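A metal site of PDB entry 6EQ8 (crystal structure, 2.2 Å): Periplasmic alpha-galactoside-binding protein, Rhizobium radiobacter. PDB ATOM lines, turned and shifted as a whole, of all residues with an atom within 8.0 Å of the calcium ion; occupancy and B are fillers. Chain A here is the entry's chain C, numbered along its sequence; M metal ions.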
ATOM      1  N   LYS A 457     -20.394 -15.626  24.435  1.00  0.00           N
ATOM      2  CA  LYS A 457     -21.243 -15.389  25.612  1.00  0.00           C
ATOM      3  C   LYS A 457     -21.051 -16.445  26.718  1.00  0.00           C
ATOM      4  O   LYS A 457     -20.724 -17.602  26.434  1.00  0.00           O
ATOM      5  CB  LYS A 457     -22.731 -15.214  25.243  1.00  0.00           C
ATOM      6  CG  LYS A 457     -23.442 -16.453  24.703  1.00  0.00           C
ATOM      7  CD  LYS A 457     -24.924 -16.171  24.487  1.00  0.00           C
ATOM      8  CE  LYS A 457     -25.754 -17.415  24.399  1.00  0.00           C
ATOM      9  NZ  LYS A 457     -27.156 -17.091  24.034  1.00  0.00           N
ATOM     10  N   ASP A 458     -21.245 -16.022  27.981  1.00  0.00           N
ATOM     11  CA  ASP A 458     -21.146 -16.899  29.138  1.00  0.00           C
ATOM     12  C   ASP A 458     -22.430 -17.743  29.230  1.00  0.00           C
ATOM     13  O   ASP A 458     -23.492 -17.238  29.594  1.00  0.00           O
ATOM     14  CB  ASP A 458     -20.869 -16.084  30.420  1.00  0.00           C
ATOM     15  CG  ASP A 458     -20.821 -16.884  31.712  1.00  0.00           C
ATOM     16  OD1 ASP A 458     -20.520 -18.105  31.653  1.00  0.00           O
ATOM     17  OD2 ASP A 458     -21.060 -16.299  32.781  1.00  0.00           O
ATOM     18  N   THR A 459     -22.313 -19.035  28.850  1.00  0.00           N
ATOM     19  CA  THR A 459     -23.429 -19.986  28.783  1.00  0.00           C
ATOM     20  C   THR A 459     -23.563 -20.882  30.033  1.00  0.00           C
ATOM     21  O   THR A 459     -24.582 -21.558  30.171  1.00  0.00           O
ATOM     22  CB  THR A 459     -23.331 -20.822  27.490  1.00  0.00           C
ATOM     23  OG1 THR A 459     -22.129 -21.589  27.476  1.00  0.00           O
ATOM     24  CG2 THR A 459     -23.435 -19.963  26.221  1.00  0.00           C
ATOM     25  N   ASP A 460     -22.548 -20.894  30.948  1.00  0.00           N
ATOM     26  CA  ASP A 460     -22.558 -21.714  32.178  1.00  0.00           C
ATOM     27  C   ASP A 460     -22.588 -20.876  33.491  1.00  0.00           C
ATOM     28  O   ASP A 460     -22.607 -21.459  34.586  1.00  0.00           O
ATOM     29  CB  ASP A 460     -21.412 -22.752  32.238  1.00  0.00           C
ATOM     30  CG  ASP A 460     -20.523 -22.980  31.031  1.00  0.00           C
ATOM     31  OD1 ASP A 460     -21.064 -23.253  29.934  1.00  0.00           O
ATOM     32  OD2 ASP A 460     -19.273 -23.001  31.202  1.00  0.00           O
ATOM     33  N   GLY A 461     -22.580 -19.555  33.374  1.00  0.00           N
ATOM     34  CA  GLY A 461     -22.667 -18.642  34.509  1.00  0.00           C
ATOM     35  C   GLY A 461     -21.439 -18.494  35.406  1.00  0.00           C
ATOM     36  O   GLY A 461     -21.592 -18.130  36.575  1.00  0.00           O
ATOM     37  N   ASP A 462     -20.231 -18.732  34.872  1.00  0.00           N
ATOM     38  CA  ASP A 462     -19.001 -18.573  35.671  1.00  0.00           C
ATOM     39  C   ASP A 462     -18.271 -17.234  35.447  1.00  0.00           C
ATOM     40  O   ASP A 462     -17.220 -17.001  36.059  1.00  0.00           O
ATOM     41  CB  ASP A 462     -18.051 -19.778  35.471  1.00  0.00           C
ATOM     42  CG  ASP A 462     -17.491 -19.998  34.076  1.00  0.00           C
ATOM     43  OD1 ASP A 462     -17.912 -19.280  33.136  1.00  0.00           O
ATOM     44  OD2 ASP A 462     -16.630 -20.887  33.918  1.00  0.00           O
ATOM     45  N   GLY A 463     -18.820 -16.381  34.583  1.00  0.00           N
ATOM     46  CA  GLY A 463     -18.219 -15.089  34.268  1.00  0.00           C
ATOM     47  C   GLY A 463     -17.328 -15.108  33.048  1.00  0.00           C
ATOM     48  O   GLY A 463     -17.021 -14.058  32.467  1.00  0.00           O
ATOM     49  N   PHE A 464     -16.884 -16.308  32.635  1.00  0.00           N
ATOM     50  CA  PHE A 464     -16.038 -16.482  31.461  1.00  0.00           C
ATOM     51  C   PHE A 464     -16.868 -16.798  30.227  1.00  0.00           C
ATOM     52  O   PHE A 464     -17.822 -17.573  30.291  1.00  0.00           O
ATOM     53  CB  PHE A 464     -14.994 -17.569  31.715  1.00  0.00           C
ATOM     54  CG  PHE A 464     -13.914 -17.123  32.675  1.00  0.00           C
ATOM     55  CD1 PHE A 464     -12.852 -16.353  32.231  1.00  0.00           C
ATOM     56  CD2 PHE A 464     -13.986 -17.460  34.020  1.00  0.00           C
ATOM     57  CE1 PHE A 464     -11.866 -15.927  33.126  1.00  0.00           C
ATOM     58  CE2 PHE A 464     -12.997 -17.050  34.913  1.00  0.00           C
ATOM     59  CZ  PHE A 464     -11.929 -16.301  34.451  1.00  0.00           C
ATOM     60  N   LEU A 465     -16.513 -16.174  29.094  1.00  0.00           N
ATOM     61  CA  LEU A 465     -17.204 -16.393  27.821  1.00  0.00           C
ATOM     62  C   LEU A 465     -16.888 -17.759  27.289  1.00  0.00           C
ATOM     63  O   LEU A 465     -15.799 -18.288  27.502  1.00  0.00           O
ATOM     64  CB  LEU A 465     -16.829 -15.309  26.772  1.00  0.00           C
ATOM     65  CG  LEU A 465     -17.032 -13.845  27.169  1.00  0.00           C
ATOM     66  CD1 LEU A 465     -16.575 -12.919  26.074  1.00  0.00           C
ATOM     67  CD2 LEU A 465     -18.474 -13.565  27.565  1.00  0.00           C
ATOM     68  N   ASN A 466     -17.872 -18.333  26.612  1.00  0.00           N
ATOM     69  CA  ASN A 466     -17.797 -19.655  26.012  1.00  0.00           C
ATOM     70  C   ASN A 466     -17.885 -19.521  24.512  1.00  0.00           C
ATOM     71  O   ASN A 466     -18.467 -18.569  23.982  1.00  0.00           O
ATOM     72  CB  ASN A 466     -18.999 -20.525  26.464  1.00  0.00           C
ATOM     73  CG  ASN A 466     -19.076 -20.830  27.934  1.00  0.00           C
ATOM     74  OD1 ASN A 466     -19.470 -19.989  28.740  1.00  0.00           O
ATOM     75  ND2 ASN A 466     -18.799 -22.078  28.297  1.00  0.00           N
ATOM     76  N   PHE A 467     -17.407 -20.550  23.823  1.00  0.00           N
ATOM     77  CA  PHE A 467     -17.587 -20.686  22.396  1.00  0.00           C
ATOM     78  C   PHE A 467     -19.022 -21.236  22.219  1.00  0.00           C
ATOM     79  O   PHE A 467     -19.548 -21.845  23.167  1.00  0.00           O
ATOM     80  CB  PHE A 467     -16.580 -21.699  21.860  1.00  0.00           C
ATOM     81  CG  PHE A 467     -15.193 -21.138  21.663  1.00  0.00           C
ATOM     82  CD1 PHE A 467     -14.939 -20.171  20.690  1.00  0.00           C
ATOM     83  CD2 PHE A 467     -14.117 -21.623  22.419  1.00  0.00           C
ATOM     84  CE1 PHE A 467     -13.648 -19.685  20.487  1.00  0.00           C
ATOM     85  CE2 PHE A 467     -12.826 -21.130  22.208  1.00  0.00           C
ATOM     86  CZ  PHE A 467     -12.604 -20.171  21.254  1.00  0.00           C
ATOM     87  N   GLY A 474     -18.778 -26.116  23.279  1.00  0.00           N
ATOM     88  CA  GLY A 474     -19.269 -24.952  24.009  1.00  0.00           C
ATOM     89  C   GLY A 474     -18.467 -24.593  25.241  1.00  0.00           C
ATOM     90  O   GLY A 474     -18.984 -23.956  26.165  1.00  0.00           O
ATOM     91  N   ARG A 475     -17.201 -25.036  25.257  1.00  0.00           N
ATOM     92  CA  ARG A 475     -16.203 -24.854  26.308  1.00  0.00           C
ATOM     93  C   ARG A 475     -15.871 -23.368  26.510  1.00  0.00           C
ATOM     94  O   ARG A 475     -16.028 -22.573  25.574  1.00  0.00           O
ATOM     95  CB  ARG A 475     -14.920 -25.552  25.845  1.00  0.00           C
ATOM     96  CG  ARG A 475     -14.261 -26.512  26.821  1.00  0.00           C
ATOM     97  CD  ARG A 475     -12.893 -26.866  26.298  1.00  0.00           C
ATOM     98  NE  ARG A 475     -12.906 -27.868  25.226  1.00  0.00           N
ATOM     99  CZ  ARG A 475     -11.836 -28.265  24.539  1.00  0.00           C
ATOM    100  NH1 ARG A 475     -10.643 -27.732  24.782  1.00  0.00           N
ATOM    101  NH2 ARG A 475     -11.950 -29.192  23.599  1.00  0.00           N
ATOM    102  N   ASN A 476     -15.402 -23.003  27.728  1.00  0.00           N
ATOM    103  CA  ASN A 476     -14.944 -21.635  28.006  1.00  0.00           C
ATOM    104  C   ASN A 476     -13.735 -21.322  27.122  1.00  0.00           C
ATOM    105  O   ASN A 476     -12.869 -22.195  26.925  1.00  0.00           O
ATOM    106  CB  ASN A 476     -14.535 -21.465  29.463  1.00  0.00           C
ATOM    107  CG  ASN A 476     -15.669 -21.213  30.407  1.00  0.00           C
ATOM    108  OD1 ASN A 476     -16.493 -20.318  30.205  1.00  0.00           O
ATOM    109  ND2 ASN A 476     -15.699 -21.955  31.490  1.00  0.00           N
ATOM    110  N   VAL A 477     -13.692 -20.089  26.572  1.00  0.00           N
ATOM    111  CA  VAL A 477     -12.595 -19.599  25.724  1.00  0.00           C
ATOM    112  C   VAL A 477     -11.286 -19.605  26.539  1.00  0.00           C
ATOM    113  O   VAL A 477     -11.269 -19.096  27.660  1.00  0.00           O
ATOM    114  CB  VAL A 477     -12.932 -18.194  25.135  1.00  0.00           C
ATOM    115  CG1 VAL A 477     -11.833 -17.692  24.188  1.00  0.00           C
ATOM    116  CG2 VAL A 477     -14.311 -18.206  24.436  1.00  0.00           C
ATOM    117  N   GLY A 505     -13.961 -11.240  30.333  1.00  0.00           N
ATOM    118  CA  GLY A 505     -14.552 -12.585  30.287  1.00  0.00           C
ATOM    119  C   GLY A 505     -13.689 -13.628  29.606  1.00  0.00           C
ATOM    120  O   GLY A 505     -14.148 -14.749  29.379  1.00  0.00           O
ATOM    121  N   ARG A 507     -10.407 -16.162  29.482  1.00  0.00           N
ATOM    122  CA  ARG A 507      -9.443 -16.901  30.296  1.00  0.00           C
ATOM    123  C   ARG A 507      -8.094 -17.006  29.566  1.00  0.00           C
ATOM    124  O   ARG A 507      -7.998 -17.620  28.504  1.00  0.00           O
ATOM    125  CB  ARG A 507      -9.950 -18.291  30.730  1.00  0.00           C
ATOM    126  CG  ARG A 507      -9.583 -18.593  32.187  1.00  0.00           C
ATOM    127  CD  ARG A 507      -9.334 -20.062  32.481  1.00  0.00           C
ATOM    128  NE  ARG A 507     -10.526 -20.894  32.343  1.00  0.00           N
ATOM    129  CZ  ARG A 507     -11.457 -21.044  33.283  1.00  0.00           C
ATOM    130  NH1 ARG A 507     -11.366 -20.386  34.437  1.00  0.00           N
ATOM    131  NH2 ARG A 507     -12.508 -21.839  33.065  1.00  0.00           N
HETATM  132 CA    CA M   1     -18.714 -19.558  30.905  1.00  0.00          CA
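The backbone carbonyl oxygen (O) of Phe 464 binds the calcium ion (2.3 Å).
OD1 of Asn 466 binds the calcium ion (2.3 Å).
OD1 of Asp 462 binds the calcium ion (2.4 Å).
The side-chain carboxylate (OD1) of Asp 458 binds the calcium ion.
OD1 of Asn 476 is bound to the calcium ion, at 2.4 Å.
The calcium ion has five donor atoms within binding distance.
ND2 of Asn 466 is in hydrogen-bond range of OD1 of Asp 460, 3.0 Å away.
The side-chain amide nitrogen (ND2) of Asn 466 lies close to the side-chain hydroxyl (OG1) of Thr 459 (3.5 Å).
The backbone NH of Asn 466 sits at hydrogen-bond distance from the backbone carbonyl oxygen of Lys 457 (2.9 Å).
O of Gly 474 is in hydrogen-bond range of ND2 of Asn 466 (2.8 Å).
N of Gly 461 lies close to OD1 of Asp 458.
The side-chain carboxylate (OD2) of Asp 458 is in hydrogen-bond range of the backbone NH (N) of Gly 463, 2.9 Å away.
The backbone carbonyl oxygen of Leu 465 lies close to the side-chain amide oxygen of Asn 476 (3.5 Å).
The side-chain carboxylate of Asp 460 lies within hydrogen-bond range of the side-chain hydroxyl of Thr 459 (3.2 Å).
Residues that only touch the calcium ion: Asp 460 (3.5 Å).
Within 4 Å of the calcium ion: Asp 458, Asp 460, Asp 462, Phe 464, Asn 466 and Asn 476.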
